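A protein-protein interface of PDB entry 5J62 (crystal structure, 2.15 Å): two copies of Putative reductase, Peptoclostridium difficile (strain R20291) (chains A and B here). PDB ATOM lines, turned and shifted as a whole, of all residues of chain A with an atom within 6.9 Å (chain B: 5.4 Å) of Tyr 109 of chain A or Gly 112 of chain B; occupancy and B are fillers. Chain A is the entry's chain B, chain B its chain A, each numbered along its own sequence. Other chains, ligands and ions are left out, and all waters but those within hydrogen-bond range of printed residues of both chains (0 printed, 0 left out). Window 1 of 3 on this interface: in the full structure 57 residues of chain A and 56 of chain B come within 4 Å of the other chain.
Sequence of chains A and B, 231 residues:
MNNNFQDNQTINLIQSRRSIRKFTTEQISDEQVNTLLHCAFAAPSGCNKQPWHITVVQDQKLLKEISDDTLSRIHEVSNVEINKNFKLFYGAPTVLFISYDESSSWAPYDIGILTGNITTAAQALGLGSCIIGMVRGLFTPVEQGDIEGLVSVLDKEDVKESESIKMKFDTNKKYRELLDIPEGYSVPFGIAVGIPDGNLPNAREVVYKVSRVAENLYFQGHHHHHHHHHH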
ATOM      1  N   PRO A  44      21.377 -22.886  27.003  1.00  0.00           N
ATOM      2  CA  PRO A  44      20.221 -23.652  26.636  1.00  0.00           C
ATOM      3  C   PRO A  44      20.543 -25.143  26.626  1.00  0.00           C
ATOM      4  O   PRO A  44      21.686 -25.523  26.456  1.00  0.00           O
ATOM      5  CB  PRO A  44      19.882 -23.184  25.221  1.00  0.00           C
ATOM      6  CG  PRO A  44      20.898 -22.173  24.849  1.00  0.00           C
ATOM      7  CD  PRO A  44      22.005 -22.220  25.859  1.00  0.00           C
ATOM      8  N   TYR A 100      29.880 -35.223  29.433  1.00  0.00           N
ATOM      9  CA  TYR A 100      28.421 -35.221  29.236  1.00  0.00           C
ATOM     10  C   TYR A 100      27.824 -36.575  29.068  1.00  0.00           C
ATOM     11  O   TYR A 100      28.478 -37.487  28.639  1.00  0.00           O
ATOM     12  CB  TYR A 100      28.043 -34.375  27.977  1.00  0.00           C
ATOM     13  CG  TYR A 100      28.372 -34.972  26.620  1.00  0.00           C
ATOM     14  CD1 TYR A 100      29.597 -34.743  26.050  1.00  0.00           C
ATOM     15  CD2 TYR A 100      27.466 -35.744  25.909  1.00  0.00           C
ATOM     16  CE1 TYR A 100      29.943 -35.275  24.841  1.00  0.00           C
ATOM     17  CE2 TYR A 100      27.814 -36.295  24.664  1.00  0.00           C
ATOM     18  CZ  TYR A 100      29.049 -36.044  24.142  1.00  0.00           C
ATOM     19  OH  TYR A 100      29.484 -36.506  22.937  1.00  0.00           O
ATOM     20  N   SER A 105      20.098 -37.342  23.391  1.00  0.00           N
ATOM     21  CA  SER A 105      20.317 -37.042  21.989  1.00  0.00           C
ATOM     22  C   SER A 105      20.786 -35.616  21.657  1.00  0.00           C
ATOM     23  O   SER A 105      21.430 -35.412  20.658  1.00  0.00           O
ATOM     24  CB  SER A 105      18.979 -37.253  21.269  1.00  0.00           C
ATOM     25  OG  SER A 105      18.561 -38.582  21.448  1.00  0.00           O
ATOM     26  N   TRP A 106      20.391 -34.627  22.456  1.00  0.00           N
ATOM     27  CA  TRP A 106      20.742 -33.235  22.228  1.00  0.00           C
ATOM     28  C   TRP A 106      22.092 -32.883  22.838  1.00  0.00           C
ATOM     29  O   TRP A 106      22.677 -31.825  22.509  1.00  0.00           O
ATOM     30  CB  TRP A 106      19.597 -32.296  22.660  1.00  0.00           C
ATOM     31  CG  TRP A 106      18.252 -32.592  22.008  1.00  0.00           C
ATOM     32  CD1 TRP A 106      17.141 -33.136  22.632  1.00  0.00           C
ATOM     33  CD2 TRP A 106      17.897 -32.492  20.601  1.00  0.00           C
ATOM     34  NE1 TRP A 106      16.098 -33.292  21.723  1.00  0.00           N
ATOM     35  CE2 TRP A 106      16.537 -32.901  20.480  1.00  0.00           C
ATOM     36  CE3 TRP A 106      18.552 -32.007  19.470  1.00  0.00           C
ATOM     37  CZ2 TRP A 106      15.861 -32.874  19.283  1.00  0.00           C
ATOM     38  CZ3 TRP A 106      17.891 -31.981  18.260  1.00  0.00           C
ATOM     39  CH2 TRP A 106      16.551 -32.427  18.163  1.00  0.00           C
ATOM     40  N   ALA A 107      22.637 -33.770  23.682  1.00  0.00           N
ATOM     41  CA  ALA A 107      23.785 -33.403  24.522  1.00  0.00           C
ATOM     42  C   ALA A 107      25.057 -32.847  23.840  1.00  0.00           C
ATOM     43  O   ALA A 107      25.713 -31.974  24.375  1.00  0.00           O
ATOM     44  CB  ALA A 107      24.178 -34.561  25.422  1.00  0.00           C
ATOM     45  N   PRO A 108      25.427 -33.392  22.679  1.00  0.00           N
ATOM     46  CA  PRO A 108      26.639 -32.838  22.038  1.00  0.00           C
ATOM     47  C   PRO A 108      26.450 -31.394  21.639  1.00  0.00           C
ATOM     48  O   PRO A 108      27.358 -30.589  21.789  1.00  0.00           O
ATOM     49  CB  PRO A 108      26.864 -33.742  20.836  1.00  0.00           C
ATOM     50  CG  PRO A 108      26.077 -35.011  21.140  1.00  0.00           C
ATOM     51  CD  PRO A 108      24.916 -34.600  22.019  1.00  0.00           C
ATOM     52  N   TYR A 109      25.230 -31.039  21.233  1.00  0.00           N
ATOM     53  CA  TYR A 109      24.986 -29.673  20.865  1.00  0.00           C
ATOM     54  C   TYR A 109      24.968 -28.812  22.114  1.00  0.00           C
ATOM     55  O   TYR A 109      25.576 -27.721  22.107  1.00  0.00           O
ATOM     56  CB  TYR A 109      23.697 -29.548  20.071  1.00  0.00           C
ATOM     57  CG  TYR A 109      23.565 -30.593  18.984  1.00  0.00           C
ATOM     58  CD1 TYR A 109      24.484 -30.682  17.982  1.00  0.00           C
ATOM     59  CD2 TYR A 109      22.508 -31.485  18.975  1.00  0.00           C
ATOM     60  CE1 TYR A 109      24.387 -31.648  16.979  1.00  0.00           C
ATOM     61  CE2 TYR A 109      22.389 -32.461  17.981  1.00  0.00           C
ATOM     62  CZ  TYR A 109      23.345 -32.543  17.000  1.00  0.00           C
ATOM     63  OH  TYR A 109      23.244 -33.480  16.016  1.00  0.00           O
ATOM     64  N   ASP A 110      24.302 -29.278  23.180  1.00  0.00           N
ATOM     65  CA  ASP A 110      24.235 -28.576  24.462  1.00  0.00           C
ATOM     66  C   ASP A 110      25.644 -28.230  24.907  1.00  0.00           C
ATOM     67  O   ASP A 110      25.917 -27.102  25.379  1.00  0.00           O
ATOM     68  CB  ASP A 110      23.605 -29.370  25.608  1.00  0.00           C
ATOM     69  CG  ASP A 110      22.160 -29.747  25.388  1.00  0.00           C
ATOM     70  OD1 ASP A 110      21.540 -29.288  24.434  1.00  0.00           O
ATOM     71  OD2 ASP A 110      21.624 -30.517  26.236  1.00  0.00           O
ATOM     72  N   ILE A 111      26.512 -29.212  24.832  1.00  0.00           N
ATOM     73  CA  ILE A 111      27.884 -29.078  25.320  1.00  0.00           C
ATOM     74  C   ILE A 111      28.679 -28.058  24.497  1.00  0.00           C
ATOM     75  O   ILE A 111      29.559 -27.411  25.027  1.00  0.00           O
ATOM     76  CB  ILE A 111      28.571 -30.520  25.436  1.00  0.00           C
ATOM     77  CG1 ILE A 111      28.730 -30.863  26.870  1.00  0.00           C
ATOM     78  CG2 ILE A 111      29.956 -30.625  24.840  1.00  0.00           C
ATOM     79  CD1 ILE A 111      27.385 -31.153  27.453  1.00  0.00           C
ATOM     80  N   GLY A 112      28.448 -28.010  23.188  1.00  0.00           N
ATOM     81  CA  GLY A 112      29.048 -26.949  22.330  1.00  0.00           C
ATOM     82  C   GLY A 112      28.615 -25.541  22.818  1.00  0.00           C
ATOM     83  O   GLY A 112      29.411 -24.636  22.923  1.00  0.00           O
ATOM     84  N   ILE A 113      27.342 -25.396  23.124  1.00  0.00           N
ATOM     85  CA  ILE A 113      26.800 -24.115  23.555  1.00  0.00           C
ATOM     86  C   ILE A 113      27.353 -23.739  24.911  1.00  0.00           C
ATOM     87  O   ILE A 113      27.814 -22.605  25.094  1.00  0.00           O
ATOM     88  CB  ILE A 113      25.278 -24.069  23.613  1.00  0.00           C
ATOM     89  CG1 ILE A 113      24.642 -24.468  22.295  1.00  0.00           C
ATOM     90  CG2 ILE A 113      24.850 -22.646  23.939  1.00  0.00           C
ATOM     91  CD1 ILE A 113      23.181 -24.857  22.421  1.00  0.00           C
ATOM     92  N   LEU A 114      27.384 -24.709  25.836  1.00  0.00           N
ATOM     93  CA  LEU A 114      28.054 -24.494  27.087  1.00  0.00           C
ATOM     94  C   LEU A 114      29.490 -24.030  26.887  1.00  0.00           C
ATOM     95  O   LEU A 114      29.945 -23.073  27.534  1.00  0.00           O
ATOM     96  CB  LEU A 114      27.998 -25.731  27.920  1.00  0.00           C
ATOM     97  CG  LEU A 114      28.766 -25.690  29.223  1.00  0.00           C
ATOM     98  CD1 LEU A 114      28.038 -26.442  30.353  1.00  0.00           C
ATOM     99  CD2 LEU A 114      30.176 -26.235  29.122  1.00  0.00           C
ATOM    100  N   THR A 115      30.208 -24.718  26.015  1.00  0.00           N
ATOM    101  CA  THR A 115      31.607 -24.355  25.705  1.00  0.00           C
ATOM    102  C   THR A 115      31.785 -22.956  25.087  1.00  0.00           C
ATOM    103  O   THR A 115      32.748 -22.206  25.408  1.00  0.00           O
ATOM    104  CB  THR A 115      32.205 -25.423  24.790  1.00  0.00           C
ATOM    105  OG1 THR A 115      32.233 -26.674  25.509  1.00  0.00           O
ATOM    106  CG2 THR A 115      33.617 -25.040  24.326  1.00  0.00           C
ATOM    107  N   GLY A 116      30.869 -22.594  24.230  1.00  0.00           N
ATOM    108  CA  GLY A 116      30.807 -21.227  23.710  1.00  0.00           C
ATOM    109  C   GLY A 116      30.567 -20.161  24.786  1.00  0.00           C
ATOM    110  O   GLY A 116      31.138 -19.096  24.740  1.00  0.00           O
ATOM    111  N   TYR B 100      25.518 -29.651   9.519  1.00  0.00           N
ATOM    112  CA  TYR B 100      26.876 -30.009   9.757  1.00  0.00           C
ATOM    113  C   TYR B 100      27.296 -31.299   9.056  1.00  0.00           C
ATOM    114  O   TYR B 100      26.480 -32.165   8.700  1.00  0.00           O
ATOM    115  CB  TYR B 100      27.183 -30.107  11.270  1.00  0.00           C
ATOM    116  CG  TYR B 100      26.685 -31.386  11.927  1.00  0.00           C
ATOM    117  CD1 TYR B 100      27.533 -32.496  12.053  1.00  0.00           C
ATOM    118  CD2 TYR B 100      25.414 -31.488  12.433  1.00  0.00           C
ATOM    119  CE1 TYR B 100      27.092 -33.681  12.630  1.00  0.00           C
ATOM    120  CE2 TYR B 100      24.922 -32.681  13.084  1.00  0.00           C
ATOM    121  CZ  TYR B 100      25.771 -33.756  13.190  1.00  0.00           C
ATOM    122  OH  TYR B 100      25.350 -34.945  13.742  1.00  0.00           O
ATOM    123  N   ALA B 107      32.265 -31.867  14.745  1.00  0.00           N
ATOM    124  CA  ALA B 107      31.269 -31.023  14.144  1.00  0.00           C
ATOM    125  C   ALA B 107      30.020 -30.808  15.007  1.00  0.00           C
ATOM    126  O   ALA B 107      29.518 -29.733  15.041  1.00  0.00           O
ATOM    127  CB  ALA B 107      30.903 -31.561  12.750  1.00  0.00           C
ATOM    128  N   PRO B 108      29.517 -31.825  15.711  1.00  0.00           N
ATOM    129  CA  PRO B 108      28.330 -31.560  16.549  1.00  0.00           C
ATOM    130  C   PRO B 108      28.627 -30.554  17.672  1.00  0.00           C
ATOM    131  O   PRO B 108      27.774 -29.752  18.020  1.00  0.00           O
ATOM    132  CB  PRO B 108      28.030 -32.959  17.147  1.00  0.00           C
ATOM    133  CG  PRO B 108      28.587 -33.909  16.139  1.00  0.00           C
ATOM    134  CD  PRO B 108      29.881 -33.243  15.727  1.00  0.00           C
ATOM    135  N   TYR B 109      29.850 -30.596  18.223  1.00  0.00           N
ATOM    136  CA  TYR B 109      30.288 -29.667  19.243  1.00  0.00           C
ATOM    137  C   TYR B 109      30.481 -28.323  18.610  1.00  0.00           C
ATOM    138  O   TYR B 109      30.053 -27.339  19.176  1.00  0.00           O
ATOM    139  CB  TYR B 109      31.576 -30.122  19.922  1.00  0.00           C
ATOM    140  CG  TYR B 109      31.537 -31.554  20.402  1.00  0.00           C
ATOM    141  CD1 TYR B 109      30.638 -31.963  21.335  1.00  0.00           C
ATOM    142  CD2 TYR B 109      32.429 -32.495  19.901  1.00  0.00           C
ATOM    143  CE1 TYR B 109      30.613 -33.290  21.771  1.00  0.00           C
ATOM    144  CE2 TYR B 109      32.415 -33.827  20.301  1.00  0.00           C
ATOM    145  CZ  TYR B 109      31.498 -34.218  21.216  1.00  0.00           C
ATOM    146  OH  TYR B 109      31.520 -35.493  21.606  1.00  0.00           O
ATOM    147  N   ASP B 110      31.125 -28.293  17.435  1.00  0.00           N
ATOM    148  CA  ASP B 110      31.358 -27.060  16.708  1.00  0.00           C
ATOM    149  C   ASP B 110      30.109 -26.268  16.457  1.00  0.00           C
ATOM    150  O   ASP B 110      30.130 -25.044  16.645  1.00  0.00           O
ATOM    151  CB  ASP B 110      31.997 -27.263  15.338  1.00  0.00           C
ATOM    152  CG  ASP B 110      33.418 -27.918  15.393  1.00  0.00           C
ATOM    153  OD1 ASP B 110      34.185 -27.806  16.387  1.00  0.00           O
ATOM    154  OD2 ASP B 110      33.740 -28.569  14.390  1.00  0.00           O
ATOM    155  N   ILE B 111      29.030 -26.909  16.020  1.00  0.00           N
ATOM    156  CA  ILE B 111      27.825 -26.175  15.760  1.00  0.00           C
ATOM    157  C   ILE B 111      27.074 -25.750  17.022  1.00  0.00           C
ATOM    158  O   ILE B 111      26.326 -24.775  16.988  1.00  0.00           O
ATOM    159  CB  ILE B 111      26.881 -26.882  14.815  1.00  0.00           C
ATOM    160  CG1 ILE B 111      26.329 -28.180  15.365  1.00  0.00           C
ATOM    161  CG2 ILE B 111      27.559 -27.087  13.456  1.00  0.00           C
ATOM    162  CD1 ILE B 111      25.081 -28.621  14.589  1.00  0.00           C
ATOM    163  N   GLY B 112      27.261 -26.451  18.127  1.00  0.00           N
ATOM    164  CA  GLY B 112      26.796 -25.904  19.382  1.00  0.00           C
ATOM    165  C   GLY B 112      27.480 -24.603  19.721  1.00  0.00           C
ATOM    166  O   GLY B 112      26.821 -23.621  20.190  1.00  0.00           O
ATOM    167  N   ILE B 113      28.796 -24.539  19.491  1.00  0.00           N
ATOM    168  CA  ILE B 113      29.516 -23.307  19.832  1.00  0.00           C
ATOM    169  C   ILE B 113      28.999 -22.189  18.939  1.00  0.00           C
ATOM    170  O   ILE B 113      28.704 -21.074  19.400  1.00  0.00           O
ATOM    171  CB  ILE B 113      31.057 -23.429  19.738  1.00  0.00           C
ATOM    172  CG1 ILE B 113      31.557 -24.527  20.654  1.00  0.00           C
ATOM    173  CG2 ILE B 113      31.671 -22.087  20.101  1.00  0.00           C
ATOM    174  CD1 ILE B 113      32.914 -25.069  20.258  1.00  0.00           C
ATOM    175  N   LEU B 114      28.902 -22.471  17.649  1.00  0.00           N
ATOM    176  CA  LEU B 114      28.341 -21.552  16.690  1.00  0.00           C
ATOM    177  C   LEU B 114      26.915 -21.050  17.070  1.00  0.00           C
ATOM    178  O   LEU B 114      26.604 -19.843  16.919  1.00  0.00           O
ATOM    179  CB  LEU B 114      28.309 -22.209  15.325  1.00  0.00           C
ATOM    180  CG  LEU B 114      27.625 -21.408  14.199  1.00  0.00           C
ATOM    181  CD1 LEU B 114      28.345 -21.655  12.847  1.00  0.00           C
ATOM    182  CD2 LEU B 114      26.186 -21.878  14.069  1.00  0.00           C
ATOM    183  N   THR B 115      26.094 -21.962  17.560  1.00  0.00           N
ATOM    184  CA  THR B 115      24.739 -21.672  18.009  1.00  0.00           C
ATOM    185  C   THR B 115      24.769 -20.751  19.251  1.00  0.00           C
ATOM    186  O   THR B 115      23.933 -19.880  19.405  1.00  0.00           O
ATOM    187  CB  THR B 115      23.997 -23.003  18.221  1.00  0.00           C
ATOM    188  OG1 THR B 115      23.851 -23.623  16.922  1.00  0.00           O
ATOM    189  CG2 THR B 115      22.619 -22.773  18.860  1.00  0.00           C
ATOM    190  N   GLY B 116      25.734 -20.957  20.101  1.00  0.00           N
ATOM    191  CA  GLY B 116      25.948 -20.115  21.276  1.00  0.00           C
ATOM    192  C   GLY B 116      26.315 -18.685  20.857  1.00  0.00           C
ATOM    193  O   GLY B 116      25.825 -17.693  21.400  1.00  0.00           O
ATOM    194  N   ASN B 117      27.184 -18.566  19.892  1.00  0.00           N
ATOM    195  CA  ASN B 117      27.468 -17.228  19.341  1.00  0.00           C
ATOM    196  C   ASN B 117      26.230 -16.538  18.794  1.00  0.00           C
ATOM    197  O   ASN B 117      26.051 -15.364  19.022  1.00  0.00           O
ATOM    198  CB  ASN B 117      28.472 -17.285  18.223  1.00  0.00           C
ATOM    199  CG  ASN B 117      29.891 -17.468  18.707  1.00  0.00           C
ATOM    200  OD1 ASN B 117      30.132 -17.673  19.861  1.00  0.00           O
ATOM    201  ND2 ASN B 117      30.840 -17.426  17.772  1.00  0.00           N
ATOM    202  N   PRO B 188      20.220 -30.878  12.350  1.00  0.00           N
ATOM    203  CA  PRO B 188      19.608 -31.306  13.624  1.00  0.00           C
ATOM    204  C   PRO B 188      18.651 -30.306  14.249  1.00  0.00           C
ATOM    205  O   PRO B 188      17.784 -30.713  15.013  1.00  0.00           O
ATOM    206  CB  PRO B 188      20.838 -31.490  14.545  1.00  0.00           C
ATOM    207  CG  PRO B 188      21.895 -30.575  13.953  1.00  0.00           C
ATOM    208  CD  PRO B 188      21.669 -30.695  12.468  1.00  0.00           C
ATOM    209  N   PHE B 189      18.846 -28.999  14.008  1.00  0.00           N
ATOM    210  CA  PHE B 189      17.973 -28.023  14.562  1.00  0.00           C
ATOM    211  C   PHE B 189      18.018 -26.711  13.787  1.00  0.00           C
ATOM    212  O   PHE B 189      18.944 -26.448  12.995  1.00  0.00           O
ATOM    213  CB  PHE B 189      18.308 -27.808  16.053  1.00  0.00           C
ATOM    214  CG  PHE B 189      19.734 -27.423  16.318  1.00  0.00           C
ATOM    215  CD1 PHE B 189      20.642 -28.355  16.806  1.00  0.00           C
ATOM    216  CD2 PHE B 189      20.170 -26.162  16.093  1.00  0.00           C
ATOM    217  CE1 PHE B 189      21.951 -28.012  17.028  1.00  0.00           C
ATOM    218  CE2 PHE B 189      21.489 -25.772  16.334  1.00  0.00           C
ATOM    219  CZ  PHE B 189      22.372 -26.690  16.787  1.00  0.00           C
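The side-chain hydroxyl of Tyr 100 of chain B lies within hydrogen-bond range of the side-chain hydroxyl of Tyr 109 of chain A, 3.4 Å away. The side-chain hydroxyl (OH) of Tyr 100 of chain A sits at hydrogen-bond distance from the side-chain hydroxyl (OH) of Tyr 109 of chain B (2.6 Å). N of Ile 113 of chain A sits close to O of Gly 112 of chain B, at 3.5 Å. The backbone carbonyl oxygen of Gly 112 of chain A sits close to the backbone NH of Ile 113 of chain B, 3.5 Å away.
O of Ile 111 of chain B lies within hydrogen-bond range of OG1 of Thr 115 of chain B (2.7 Å). O of Ile 111 of chain A is in hydrogen-bond range of OG1 of Thr 115 of chain A (2.8 Å).
Among the printed residues, pairs that only touch across the chains: Gly 112 of chain A with Tyr 109 of chain B (3.3 Å), Tyr 109 of chain A with Pro 108 of chain B (3.4 Å), Gly 112 of chain A with Gly 112 of chain B (3.4 Å), Tyr 109 of chain A with Pro 188 of chain B (3.5 Å), Trp 106 of chain A with Pro 188 of chain B (3.5 Å), Tyr 109 of chain A with Gly 112 of chain B (3.5 Å), Pro 108 of chain A with Tyr 109 of chain B (3.6 Å), Tyr 109 of chain A with Phe 189 of chain B (3.6 Å), Gly 116 of chain A with Ile 113 of chain B (3.8 Å), Ile 111 of chain A with Tyr 109 of chain B (3.8 Å), Ile 113 of chain A with Gly 116 of chain B (3.8 Å), Pro 108 of chain A with Pro 108 of chain B (3.9 Å) and Tyr 109 of chain A with Ile 111 of chain B (3.9 Å).
Printed residues of chain B within 4 Å of Tyr 109 of chain A: Tyr 100, Pro 108, Ile 111, Gly 112, Pro 188 and Phe 189. Printed residues of chain A within 4 Å of Tyr 100 of chain B: Tyr 109. Of chain A, only Tyr 109, Gly 112 and Ile 113 come within 4 Å of Gly 112 of chain B. Printed residues of chain A within 4 Å of Phe 189 of chain B: Tyr 109. The nearest residue of chain A that does not touch Gly 112 of chain B is Pro 108 of chain A (5.3 Å).
Of the 14 printed residues of chain B, 9 touch a printed residue of chain A. Printed residues of chain B that touch a printed residue of chain A: Tyr 100, Pro 108, Tyr 109, Ile 111, Gly 112, Ile 113, Gly 116, Pro 188 and Phe 189. Hydrophobic or aromatic side chains of chain B within 4 Å of the printed part of chain A: Tyr 100, Pro 108, Tyr 109, Ile 111, Ile 113, Pro 188 and Phe 189. Among the printed residues, no Asp or Glu carboxylate lies within 4 Å of a Lys or Arg side-chain nitrogen of the other chain.
Pro 108 of chain A touches Tyr 109 of chain B, and with the chains exchanged Tyr 109 of chain A touches Pro 108 of chain B. Tyr 109 of chain A touches Gly 112 of chain B, and with the chains exchanged Gly 112 of chain A touches Tyr 109 of chain B. Gly 112 of chain B touches its own counterpart, Gly 112 of chain A. Ile 113 of chain A touches Gly 116 of chain B, and with the chains exchanged Gly 116 of chain A touches Ile 113 of chain B. Positions printed for both chains: 100, 107, 108, 109, 110, 111, 112, 113, 114, 115 and 116.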
